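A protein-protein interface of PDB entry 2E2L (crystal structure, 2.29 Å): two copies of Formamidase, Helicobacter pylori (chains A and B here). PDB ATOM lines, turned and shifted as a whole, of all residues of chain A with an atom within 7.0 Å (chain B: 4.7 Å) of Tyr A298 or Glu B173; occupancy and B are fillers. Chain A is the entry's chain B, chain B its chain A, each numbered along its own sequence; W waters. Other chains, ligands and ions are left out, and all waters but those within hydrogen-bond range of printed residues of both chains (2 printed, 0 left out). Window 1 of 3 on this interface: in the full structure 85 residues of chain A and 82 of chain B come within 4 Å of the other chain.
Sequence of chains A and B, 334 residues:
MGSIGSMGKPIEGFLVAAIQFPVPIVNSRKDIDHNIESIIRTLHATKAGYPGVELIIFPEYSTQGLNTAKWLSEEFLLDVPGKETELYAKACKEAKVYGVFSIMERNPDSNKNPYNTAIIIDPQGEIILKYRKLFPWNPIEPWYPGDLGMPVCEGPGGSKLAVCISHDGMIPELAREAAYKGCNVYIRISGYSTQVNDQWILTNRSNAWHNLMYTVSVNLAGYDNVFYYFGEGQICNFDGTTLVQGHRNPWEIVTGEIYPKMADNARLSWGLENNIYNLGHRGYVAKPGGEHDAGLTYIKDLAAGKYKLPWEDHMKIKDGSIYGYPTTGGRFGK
Pro A172 touches Arg B176.
Glu A173 touches Tyr B298 (O to CE2, 3.2 Å).
Pro B172 touches Arg A176.
His A210 touches Pro B172 (ND1 to CD, 3.7 Å).
Ile B171 touches Asn A275 (CD1 to O, 3.7 Å).
Leu A279 touches Ile B171.
Glu B173 touches Leu A279 (OE2 to CD2, 3.6 Å).
Glu B173 touches Leu A296 (CB to CD1, 3.8 Å).
Leu B279 touches Leu A302 (O to CD1, 3.6 Å).
CD2 of Leu B279 touches OH of Tyr A307, 3.7 Å away.
The guanidinium group (NE) of Arg A176 lies within salt-bridge range of the side-chain carboxylate (OE2) of Glu B173.
The guanidinium group of Arg B176 lies within salt-bridge range of the side-chain carboxylate of Glu A173 (2.8 Å).
The side-chain hydroxyl (OG1) of Thr A297 is in hydrogen-bond range of the side-chain carboxylate (OE2) of Glu B177 (2.7 Å).
The backbone NH (N) of Tyr A298 lies within hydrogen-bond range of the side-chain carboxylate (OE1) of Glu B177 (3.0 Å).
The side-chain hydroxyl of Tyr B180 lies within hydrogen-bond range of the side-chain carboxylate of Asp A301, at 2.6 Å.
N of Tyr B298 is in hydrogen-bond range of OE1 of Glu A177, 3.0 Å away.
Water W2 lies within hydrogen-bond range of the side-chain carboxylate (OE2) of Glu B177 (2.7 Å) and the backbone carbonyl oxygen (O) of Gly A295 (2.8 Å).
Water W1 lies within hydrogen-bond range of the side-chain carboxylate (OE2) of Glu A173 (2.9 Å), the backbone carbonyl oxygen (O) of Pro B172 (3.1 Å) and the backbone NH (N) of Glu B173 (3.2 Å).
Of the 10 printed residues of chain B, 9 touch a printed residue of chain A.
OE2 of Glu B173 is in hydrogen-bond range of OH of Tyr B298, 2.8 Å away.
OE2 of Glu A173 is in hydrogen-bond range of OH of Tyr A298.
The guanidinium group (NH1) of Arg A176 sits at hydrogen-bond distance from the backbone carbonyl oxygen (O) of His A210.
OD1 of Asn A211 is in hydrogen-bond range of NH1 of Arg A176.
N of Lys A306 sits at hydrogen-bond distance from O of Asp A301.
The backbone carbonyl oxygen (O) of Asp A301 sits at hydrogen-bond distance from the backbone NH (N) of Tyr A307 (3.4 Å).
Pro A172 touches Arg B176, and with the chains exchanged Arg A176 touches Pro B172.
Glu A173 touches Tyr B298, and with the chains exchanged Tyr A298 touches Glu B173.
Arg A176 touches Tyr B298, and with the chains exchanged Tyr A298 touches Arg B176.
Glu A177 touches Tyr B298, and with the chains exchanged Tyr A298 touches Glu B177.
Positions printed for both chains: 172, 173, 176, 177, 279 and 298.
Printed residues of chain B within 4 Å of Tyr A298: Glu B173, Arg B176, Glu B177 and Tyr B180.
Of chain A, only Arg A176, Leu A279, Leu A296 and Tyr A298 come within 4 Å of Glu B173.
Of the printed residues of chain A, Leu B279 touches Glu A173, Leu A302 and Tyr A307.
Of the printed residues of chain A, Tyr B180 touches Thr A297 (3.7 Å), Tyr A298 (3.5 Å), Asp A301 (2.6 Å), Lys A306 (3.8 Å) and Tyr A307 (3.5 Å).
Of the printed residues of chain A, Glu B177 touches Leu A296 (3.6 Å), Thr A297 (2.7 Å) and Tyr A298 (3.0 Å).
Printed residues of chain A within 4 Å of Ile B171: Asn A275 (3.7 Å) and Leu A279 (3.8 Å).
Ala A304 touches none of the printed residues of chain B.
Ala A303 touches none of the printed residues of chain B.
The nearest printed residue of chain B that does not touch Thr A297 is Arg B176 (7.5 Å).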
ATOM      1  N   PRO A 172     -23.252   4.286  -1.902  1.00  0.00           N
ATOM      2  CA  PRO A 172     -22.561   4.042  -3.173  1.00  0.00           C
ATOM      3  C   PRO A 172     -23.140   4.841  -4.344  1.00  0.00           C
ATOM      4  O   PRO A 172     -22.395   5.244  -5.238  1.00  0.00           O
ATOM      5  CB  PRO A 172     -22.756   2.536  -3.400  1.00  0.00           C
ATOM      6  CG  PRO A 172     -23.945   2.173  -2.594  1.00  0.00           C
ATOM      7  CD  PRO A 172     -23.903   3.066  -1.395  1.00  0.00           C
ATOM      8  N   GLU A 173     -24.452   5.068  -4.327  1.00  0.00           N
ATOM      9  CA  GLU A 173     -25.124   5.865  -5.352  1.00  0.00           C
ATOM     10  C   GLU A 173     -24.558   7.283  -5.413  1.00  0.00           C
ATOM     11  O   GLU A 173     -24.442   7.867  -6.495  1.00  0.00           O
ATOM     12  CB  GLU A 173     -26.636   5.908  -5.104  1.00  0.00           C
ATOM     13  CG  GLU A 173     -27.372   4.584  -5.347  1.00  0.00           C
ATOM     14  CD  GLU A 173     -27.419   3.669  -4.128  1.00  0.00           C
ATOM     15  OE1 GLU A 173     -26.758   3.960  -3.107  1.00  0.00           O
ATOM     16  OE2 GLU A 173     -28.128   2.643  -4.199  1.00  0.00           O
ATOM     17  N   ARG A 176     -21.281   7.199  -7.165  1.00  0.00           N
ATOM     18  CA  ARG A 176     -21.591   7.078  -8.585  1.00  0.00           C
ATOM     19  C   ARG A 176     -21.954   8.435  -9.182  1.00  0.00           C
ATOM     20  O   ARG A 176     -21.532   8.751 -10.289  1.00  0.00           O
ATOM     21  CB  ARG A 176     -22.717   6.064  -8.825  1.00  0.00           C
ATOM     22  CG  ARG A 176     -23.057   5.831 -10.302  1.00  0.00           C
ATOM     23  CD  ARG A 176     -22.067   4.905 -10.984  1.00  0.00           C
ATOM     24  NE  ARG A 176     -22.320   3.507 -10.650  1.00  0.00           N
ATOM     25  CZ  ARG A 176     -21.403   2.546 -10.673  1.00  0.00           C
ATOM     26  NH1 ARG A 176     -20.149   2.822 -11.000  1.00  0.00           N
ATOM     27  NH2 ARG A 176     -21.743   1.306 -10.356  1.00  0.00           N
ATOM     28  N   GLU A 177     -22.723   9.229  -8.437  1.00  0.00           N
ATOM     29  CA  GLU A 177     -23.177  10.544  -8.901  1.00  0.00           C
ATOM     30  C   GLU A 177     -22.026  11.506  -9.183  1.00  0.00           C
ATOM     31  O   GLU A 177     -21.985  12.127 -10.246  1.00  0.00           O
ATOM     32  CB  GLU A 177     -24.179  11.159  -7.913  1.00  0.00           C
ATOM     33  CG  GLU A 177     -24.679  12.563  -8.286  1.00  0.00           C
ATOM     34  CD  GLU A 177     -25.540  12.604  -9.550  1.00  0.00           C
ATOM     35  OE1 GLU A 177     -25.750  11.553 -10.199  1.00  0.00           O
ATOM     36  OE2 GLU A 177     -26.013  13.707  -9.899  1.00  0.00           O
ATOM     37  N   HIS A 210     -15.655   1.093  -7.639  1.00  0.00           N
ATOM     38  CA  HIS A 210     -16.915   1.111  -8.392  1.00  0.00           C
ATOM     39  C   HIS A 210     -16.912   2.114  -9.540  1.00  0.00           C
ATOM     40  O   HIS A 210     -17.564   1.899 -10.563  1.00  0.00           O
ATOM     41  CB  HIS A 210     -18.101   1.425  -7.477  1.00  0.00           C
ATOM     42  CG  HIS A 210     -18.495   0.299  -6.573  1.00  0.00           C
ATOM     43  ND1 HIS A 210     -18.417  -1.024  -6.950  1.00  0.00           N
ATOM     44  CD2 HIS A 210     -19.006   0.305  -5.320  1.00  0.00           C
ATOM     45  CE1 HIS A 210     -18.841  -1.786  -5.958  1.00  0.00           C
ATOM     46  NE2 HIS A 210     -19.206  -1.005  -4.958  1.00  0.00           N
ATOM     47  N   ASN A 211     -16.168   3.201  -9.363  1.00  0.00           N
ATOM     48  CA  ASN A 211     -16.259   4.354 -10.252  1.00  0.00           C
ATOM     49  C   ASN A 211     -14.971   4.689 -10.995  1.00  0.00           C
ATOM     50  O   ASN A 211     -14.943   5.615 -11.812  1.00  0.00           O
ATOM     51  CB  ASN A 211     -16.751   5.562  -9.459  1.00  0.00           C
ATOM     52  CG  ASN A 211     -18.103   5.318  -8.815  1.00  0.00           C
ATOM     53  OD1 ASN A 211     -19.110   5.172  -9.504  1.00  0.00           O
ATOM     54  ND2 ASN A 211     -18.129   5.265  -7.487  1.00  0.00           N
ATOM     55  N   ASN A 275     -16.923  -0.961 -15.113  1.00  0.00           N
ATOM     56  CA  ASN A 275     -18.245  -1.191 -14.529  1.00  0.00           C
ATOM     57  C   ASN A 275     -19.174   0.015 -14.640  1.00  0.00           C
ATOM     58  O   ASN A 275     -20.380  -0.140 -14.846  1.00  0.00           O
ATOM     59  CB  ASN A 275     -18.112  -1.631 -13.067  1.00  0.00           C
ATOM     60  CG  ASN A 275     -17.115  -2.764 -12.884  1.00  0.00           C
ATOM     61  OD1 ASN A 275     -16.199  -2.674 -12.068  1.00  0.00           O
ATOM     62  ND2 ASN A 275     -17.283  -3.831 -13.649  1.00  0.00           N
ATOM     63  N   LEU A 279     -23.000  -0.360 -16.459  1.00  0.00           N
ATOM     64  CA  LEU A 279     -24.268  -0.067 -15.787  1.00  0.00           C
ATOM     65  C   LEU A 279     -25.329   0.531 -16.717  1.00  0.00           C
ATOM     66  O   LEU A 279     -26.513   0.215 -16.594  1.00  0.00           O
ATOM     67  CB  LEU A 279     -24.031   0.851 -14.576  1.00  0.00           C
ATOM     68  CG  LEU A 279     -25.241   1.426 -13.829  1.00  0.00           C
ATOM     69  CD1 LEU A 279     -26.077   0.330 -13.180  1.00  0.00           C
ATOM     70  CD2 LEU A 279     -24.798   2.456 -12.793  1.00  0.00           C
ATOM     71  N   ALA A 294     -31.654  -0.550 -17.131  1.00  0.00           N
ATOM     72  CA  ALA A 294     -30.911  -1.364 -16.166  1.00  0.00           C
ATOM     73  C   ALA A 294     -31.710  -2.561 -15.645  1.00  0.00           C
ATOM     74  O   ALA A 294     -31.134  -3.602 -15.325  1.00  0.00           O
ATOM     75  CB  ALA A 294     -30.415  -0.507 -15.013  1.00  0.00           C
ATOM     76  N   GLY A 295     -33.032  -2.405 -15.568  1.00  0.00           N
ATOM     77  CA  GLY A 295     -33.927  -3.471 -15.115  1.00  0.00           C
ATOM     78  C   GLY A 295     -34.134  -3.489 -13.610  1.00  0.00           C
ATOM     79  O   GLY A 295     -34.507  -4.516 -13.041  1.00  0.00           O
ATOM     80  N   LEU A 296     -33.900  -2.344 -12.972  1.00  0.00           N
ATOM     81  CA  LEU A 296     -33.963  -2.226 -11.517  1.00  0.00           C
ATOM     82  C   LEU A 296     -35.121  -1.326 -11.093  1.00  0.00           C
ATOM     83  O   LEU A 296     -35.254  -0.197 -11.575  1.00  0.00           O
ATOM     84  CB  LEU A 296     -32.634  -1.696 -10.960  1.00  0.00           C
ATOM     85  CG  LEU A 296     -31.324  -2.219 -11.568  1.00  0.00           C
ATOM     86  CD1 LEU A 296     -30.131  -1.473 -11.001  1.00  0.00           C
ATOM     87  CD2 LEU A 296     -31.156  -3.726 -11.375  1.00  0.00           C
ATOM     88  N   THR A 297     -35.954  -1.840 -10.195  1.00  0.00           N
ATOM     89  CA  THR A 297     -37.154  -1.138  -9.747  1.00  0.00           C
ATOM     90  C   THR A 297     -36.849   0.039  -8.817  1.00  0.00           C
ATOM     91  O   THR A 297     -37.529   1.066  -8.882  1.00  0.00           O
ATOM     92  CB  THR A 297     -38.153  -2.092  -9.044  1.00  0.00           C
ATOM     93  OG1 THR A 297     -37.533  -2.686  -7.896  1.00  0.00           O
ATOM     94  CG2 THR A 297     -38.631  -3.189  -9.993  1.00  0.00           C
ATOM     95  N   TYR A 298     -35.829  -0.108  -7.969  1.00  0.00           N
ATOM     96  CA  TYR A 298     -35.498   0.921  -6.974  1.00  0.00           C
ATOM     97  C   TYR A 298     -34.994   2.210  -7.624  1.00  0.00           C
ATOM     98  O   TYR A 298     -35.248   3.303  -7.114  1.00  0.00           O
ATOM     99  CB  TYR A 298     -34.500   0.398  -5.924  1.00  0.00           C
ATOM    100  CG  TYR A 298     -33.052   0.782  -6.148  1.00  0.00           C
ATOM    101  CD1 TYR A 298     -32.541   1.983  -5.644  1.00  0.00           C
ATOM    102  CD2 TYR A 298     -32.191  -0.055  -6.851  1.00  0.00           C
ATOM    103  CE1 TYR A 298     -31.215   2.340  -5.848  1.00  0.00           C
ATOM    104  CE2 TYR A 298     -30.865   0.291  -7.056  1.00  0.00           C
ATOM    105  CZ  TYR A 298     -30.381   1.485  -6.551  1.00  0.00           C
ATOM    106  OH  TYR A 298     -29.063   1.828  -6.755  1.00  0.00           O
ATOM    107  N   ILE A 299     -34.277   2.063  -8.739  1.00  0.00           N
ATOM    108  CA  ILE A 299     -33.793   3.195  -9.531  1.00  0.00           C
ATOM    109  C   ILE A 299     -34.972   4.045 -10.004  1.00  0.00           C
ATOM    110  O   ILE A 299     -34.974   5.267  -9.838  1.00  0.00           O
ATOM    111  CB  ILE A 299     -32.941   2.717 -10.746  1.00  0.00           C
ATOM    112  CG1 ILE A 299     -31.650   2.025 -10.280  1.00  0.00           C
ATOM    113  CG2 ILE A 299     -32.635   3.869 -11.709  1.00  0.00           C
ATOM    114  CD1 ILE A 299     -30.626   2.949  -9.624  1.00  0.00           C
ATOM    115  N   LYS A 300     -35.977   3.385 -10.573  1.00  0.00           N
ATOM    116  CA  LYS A 300     -37.180   4.057 -11.050  1.00  0.00           C
ATOM    117  C   LYS A 300     -38.025   4.619  -9.905  1.00  0.00           C
ATOM    118  O   LYS A 300     -38.646   5.671 -10.053  1.00  0.00           O
ATOM    119  CB  LYS A 300     -37.996   3.121 -11.944  1.00  0.00           C
ATOM    120  CG  LYS A 300     -37.354   2.904 -13.311  1.00  0.00           C
ATOM    121  CD  LYS A 300     -37.882   1.671 -14.010  1.00  0.00           C
ATOM    122  CE  LYS A 300     -37.314   1.569 -15.420  1.00  0.00           C
ATOM    123  NZ  LYS A 300     -37.512   0.209 -16.002  1.00  0.00           N
ATOM    124  N   ASP A 301     -38.028   3.927  -8.768  1.00  0.00           N
ATOM    125  CA  ASP A 301     -38.739   4.396  -7.579  1.00  0.00           C
ATOM    126  C   ASP A 301     -38.077   5.617  -6.943  1.00  0.00           C
ATOM    127  O   ASP A 301     -38.752   6.588  -6.605  1.00  0.00           O
ATOM    128  CB  ASP A 301     -38.882   3.273  -6.546  1.00  0.00           C
ATOM    129  CG  ASP A 301     -39.909   2.223  -6.952  1.00  0.00           C
ATOM    130  OD1 ASP A 301     -40.483   2.321  -8.058  1.00  0.00           O
ATOM    131  OD2 ASP A 301     -40.141   1.293  -6.153  1.00  0.00           O
ATOM    132  N   LEU A 302     -36.756   5.565  -6.789  1.00  0.00           N
ATOM    133  CA  LEU A 302     -35.999   6.659  -6.189  1.00  0.00           C
ATOM    134  C   LEU A 302     -36.005   7.905  -7.075  1.00  0.00           C
ATOM    135  O   LEU A 302     -36.007   9.026  -6.567  1.00  0.00           O
ATOM    136  CB  LEU A 302     -34.562   6.216  -5.874  1.00  0.00           C
ATOM    137  CG  LEU A 302     -33.628   7.137  -5.077  1.00  0.00           C
ATOM    138  CD1 LEU A 302     -34.142   7.408  -3.668  1.00  0.00           C
ATOM    139  CD2 LEU A 302     -32.231   6.540  -5.025  1.00  0.00           C
ATOM    140  N   ALA A 303     -36.014   7.696  -8.391  1.00  0.00           N
ATOM    141  CA  ALA A 303     -36.094   8.792  -9.361  1.00  0.00           C
ATOM    142  C   ALA A 303     -37.413   9.555  -9.253  1.00  0.00           C
ATOM    143  O   ALA A 303     -37.433  10.784  -9.355  1.00  0.00           O
ATOM    144  CB  ALA A 303     -35.894   8.272 -10.782  1.00  0.00           C
ATOM    145  N   ALA A 304     -38.503   8.818  -9.041  1.00  0.00           N
ATOM    146  CA  ALA A 304     -39.828   9.408  -8.861  1.00  0.00           C
ATOM    147  C   ALA A 304     -40.147   9.707  -7.390  1.00  0.00           C
ATOM    148  O   ALA A 304     -41.261  10.125  -7.061  1.00  0.00           O
ATOM    149  CB  ALA A 304     -40.893   8.508  -9.470  1.00  0.00           C
ATOM    150  N   LYS A 306     -40.383   7.632  -4.789  1.00  0.00           N
ATOM    151  CA  LYS A 306     -41.328   6.663  -4.230  1.00  0.00           C
ATOM    152  C   LYS A 306     -40.605   5.406  -3.720  1.00  0.00           C
ATOM    153  O   LYS A 306     -41.206   4.337  -3.570  1.00  0.00           O
ATOM    154  CB  LYS A 306     -42.418   6.319  -5.262  1.00  0.00           C
ATOM    155  CG  LYS A 306     -41.904   5.627  -6.518  1.00  0.00           C
ATOM    156  CD  LYS A 306     -42.814   5.831  -7.713  1.00  0.00           C
ATOM    157  CE  LYS A 306     -42.269   5.105  -8.937  1.00  0.00           C
ATOM    158  NZ  LYS A 306     -42.973   5.492 -10.194  1.00  0.00           N
ATOM    159  N   TYR A 307     -39.308   5.564  -3.458  1.00  0.00           N
ATOM    160  CA  TYR A 307     -38.455   4.533  -2.865  1.00  0.00           C
ATOM    161  C   TYR A 307     -38.988   4.135  -1.493  1.00  0.00           C
ATOM    162  O   TYR A 307     -38.999   4.945  -0.563  1.00  0.00           O
ATOM    163  CB  TYR A 307     -37.023   5.078  -2.751  1.00  0.00           C
ATOM    164  CG  TYR A 307     -35.981   4.146  -2.163  1.00  0.00           C
ATOM    165  CD1 TYR A 307     -35.114   3.432  -2.989  1.00  0.00           C
ATOM    166  CD2 TYR A 307     -35.831   4.011  -0.781  1.00  0.00           C
ATOM    167  CE1 TYR A 307     -34.142   2.590  -2.455  1.00  0.00           C
ATOM    168  CE2 TYR A 307     -34.865   3.172  -0.238  1.00  0.00           C
ATOM    169  CZ  TYR A 307     -34.023   2.465  -1.080  1.00  0.00           C
ATOM    170  OH  TYR A 307     -33.066   1.634  -0.546  1.00  0.00           O
ATOM    171  N   ILE B 171     -21.486  -4.355  -9.633  1.00  0.00           N
ATOM    172  CA  ILE B 171     -22.482  -3.292  -9.756  1.00  0.00           C
ATOM    173  C   ILE B 171     -23.240  -3.167  -8.430  1.00  0.00           C
ATOM    174  O   ILE B 171     -24.066  -4.024  -8.110  1.00  0.00           O
ATOM    175  CB  ILE B 171     -23.484  -3.574 -10.927  1.00  0.00           C
ATOM    176  CG1 ILE B 171     -22.752  -3.910 -12.241  1.00  0.00           C
ATOM    177  CG2 ILE B 171     -24.483  -2.421 -11.100  1.00  0.00           C
ATOM    178  CD1 ILE B 171     -21.872  -2.792 -12.810  1.00  0.00           C
ATOM    179  N   PRO B 172     -22.952  -2.107  -7.647  1.00  0.00           N
ATOM    180  CA  PRO B 172     -23.594  -1.936  -6.338  1.00  0.00           C
ATOM    181  C   PRO B 172     -25.108  -1.718  -6.416  1.00  0.00           C
ATOM    182  O   PRO B 172     -25.827  -2.089  -5.487  1.00  0.00           O
ATOM    183  CB  PRO B 172     -22.893  -0.701  -5.755  1.00  0.00           C
ATOM    184  CG  PRO B 172     -22.369   0.038  -6.937  1.00  0.00           C
ATOM    185  CD  PRO B 172     -22.004  -1.016  -7.940  1.00  0.00           C
ATOM    186  N   GLU B 173     -25.580  -1.127  -7.515  1.00  0.00           N
ATOM    187  CA  GLU B 173     -27.009  -0.899  -7.740  1.00  0.00           C
ATOM    188  C   GLU B 173     -27.790  -2.209  -7.843  1.00  0.00           C
ATOM    189  O   GLU B 173     -28.969  -2.263  -7.488  1.00  0.00           O
ATOM    190  CB  GLU B 173     -27.246  -0.059  -9.004  1.00  0.00           C
ATOM    191  CG  GLU B 173     -26.813   1.407  -8.909  1.00  0.00           C
ATOM    192  CD  GLU B 173     -25.339   1.623  -9.203  1.00  0.00           C
ATOM    193  OE1 GLU B 173     -24.605   0.629  -9.397  1.00  0.00           O
ATOM    194  OE2 GLU B 173     -24.912   2.796  -9.245  1.00  0.00           O
ATOM    195  N   LEU B 174     -27.137  -3.259  -8.333  1.00  0.00           N
ATOM    196  CA  LEU B 174     -27.772  -4.571  -8.425  1.00  0.00           C
ATOM    197  C   LEU B 174     -27.916  -5.227  -7.050  1.00  0.00           C
ATOM    198  O   LEU B 174     -28.907  -5.911  -6.787  1.00  0.00           O
ATOM    199  CB  LEU B 174     -27.021  -5.484  -9.397  1.00  0.00           C
ATOM    200  CG  LEU B 174     -27.718  -6.781  -9.828  1.00  0.00           C
ATOM    201  CD1 LEU B 174     -29.190  -6.553 -10.172  1.00  0.00           C
ATOM    202  CD2 LEU B 174     -26.995  -7.413 -11.004  1.00  0.00           C
ATOM    203  N   ALA B 175     -26.927  -5.012  -6.182  1.00  0.00           N
ATOM    204  CA  ALA B 175     -27.009  -5.461  -4.793  1.00  0.00           C
ATOM    205  C   ALA B 175     -28.107  -4.695  -4.055  1.00  0.00           C
ATOM    206  O   ALA B 175     -28.835  -5.263  -3.239  1.00  0.00           O
ATOM    207  CB  ALA B 175     -25.674  -5.289  -4.098  1.00  0.00           C
ATOM    208  N   ARG B 176     -28.221  -3.404  -4.361  1.00  0.00           N
ATOM    209  CA  ARG B 176     -29.282  -2.563  -3.821  1.00  0.00           C
ATOM    210  C   ARG B 176     -30.666  -3.058  -4.248  1.00  0.00           C
ATOM    211  O   ARG B 176     -31.585  -3.122  -3.426  1.00  0.00           O
ATOM    212  CB  ARG B 176     -29.073  -1.105  -4.245  1.00  0.00           C
ATOM    213  CG  ARG B 176     -30.028  -0.119  -3.588  1.00  0.00           C
ATOM    214  CD  ARG B 176     -29.710   0.099  -2.128  1.00  0.00           C
ATOM    215  NE  ARG B 176     -28.652   1.084  -1.944  1.00  0.00           N
ATOM    216  CZ  ARG B 176     -27.960   1.238  -0.822  1.00  0.00           C
ATOM    217  NH1 ARG B 176     -28.196   0.453   0.223  1.00  0.00           N
ATOM    218  NH2 ARG B 176     -27.023   2.170  -0.748  1.00  0.00           N
ATOM    219  N   GLU B 177     -30.795  -3.419  -5.525  1.00  0.00           N
ATOM    220  CA  GLU B 177     -32.059  -3.893  -6.087  1.00  0.00           C
ATOM    221  C   GLU B 177     -32.582  -5.150  -5.390  1.00  0.00           C
ATOM    222  O   GLU B 177     -33.760  -5.214  -5.025  1.00  0.00           O
ATOM    223  CB  GLU B 177     -31.922  -4.129  -7.599  1.00  0.00           C
ATOM    224  CG  GLU B 177     -33.164  -4.720  -8.280  1.00  0.00           C
ATOM    225  CD  GLU B 177     -34.363  -3.780  -8.294  1.00  0.00           C
ATOM    226  OE1 GLU B 177     -34.229  -2.602  -7.890  1.00  0.00           O
ATOM    227  OE2 GLU B 177     -35.450  -4.220  -8.721  1.00  0.00           O
ATOM    228  N   TYR B 180     -33.707  -4.324  -1.930  1.00  0.00           N
ATOM    229  CA  TYR B 180     -34.934  -3.537  -2.076  1.00  0.00           C
ATOM    230  C   TYR B 180     -36.159  -4.430  -2.245  1.00  0.00           C
ATOM    231  O   TYR B 180     -37.264  -4.059  -1.852  1.00  0.00           O
ATOM    232  CB  TYR B 180     -34.808  -2.599  -3.277  1.00  0.00           C
ATOM    233  CG  TYR B 180     -35.922  -1.590  -3.429  1.00  0.00           C
ATOM    234  CD1 TYR B 180     -35.983  -0.463  -2.609  1.00  0.00           C
ATOM    235  CD2 TYR B 180     -36.900  -1.742  -4.416  1.00  0.00           C
ATOM    236  CE1 TYR B 180     -36.995   0.476  -2.755  1.00  0.00           C
ATOM    237  CE2 TYR B 180     -37.918  -0.804  -4.570  1.00  0.00           C
ATOM    238  CZ  TYR B 180     -37.955   0.305  -3.734  1.00  0.00           C
ATOM    239  OH  TYR B 180     -38.955   1.243  -3.867  1.00  0.00           O
ATOM    240  N   LEU B 279     -31.050   6.187   2.190  1.00  0.00           N
ATOM    241  CA  LEU B 279     -31.045   6.477   0.752  1.00  0.00           C
ATOM    242  C   LEU B 279     -32.350   7.121   0.262  1.00  0.00           C
ATOM    243  O   LEU B 279     -32.326   8.031  -0.568  1.00  0.00           O
ATOM    244  CB  LEU B 279     -30.738   5.205  -0.054  1.00  0.00           C
ATOM    245  CG  LEU B 279     -30.787   5.249  -1.591  1.00  0.00           C
ATOM    246  CD1 LEU B 279     -29.713   6.165  -2.165  1.00  0.00           C
ATOM    247  CD2 LEU B 279     -30.658   3.855  -2.174  1.00  0.00           C
ATOM    248  N   TYR B 298     -27.905  10.928 -12.134  1.00  0.00           N
ATOM    249  CA  TYR B 298     -27.711   9.628 -12.782  1.00  0.00           C
ATOM    250  C   TYR B 298     -28.860   8.659 -12.500  1.00  0.00           C
ATOM    251  O   TYR B 298     -29.192   7.832 -13.348  1.00  0.00           O
ATOM    252  CB  TYR B 298     -26.349   9.014 -12.415  1.00  0.00           C
ATOM    253  CG  TYR B 298     -26.373   7.937 -11.349  1.00  0.00           C
ATOM    254  CD1 TYR B 298     -26.520   6.592 -11.697  1.00  0.00           C
ATOM    255  CD2 TYR B 298     -26.231   8.258 -10.001  1.00  0.00           C
ATOM    256  CE1 TYR B 298     -26.542   5.595 -10.727  1.00  0.00           C
ATOM    257  CE2 TYR B 298     -26.247   7.269  -9.023  1.00  0.00           C
ATOM    258  CZ  TYR B 298     -26.399   5.941  -9.393  1.00  0.00           C
ATOM    259  OH  TYR B 298     -26.412   4.959  -8.432  1.00  0.00           O
HETATM  260  O   HOH W   1     -25.930   0.966  -5.081  1.00  0.00           O
HETATM  261  O   HOH W   2     -35.268  -6.033 -10.759  1.00  0.00           O
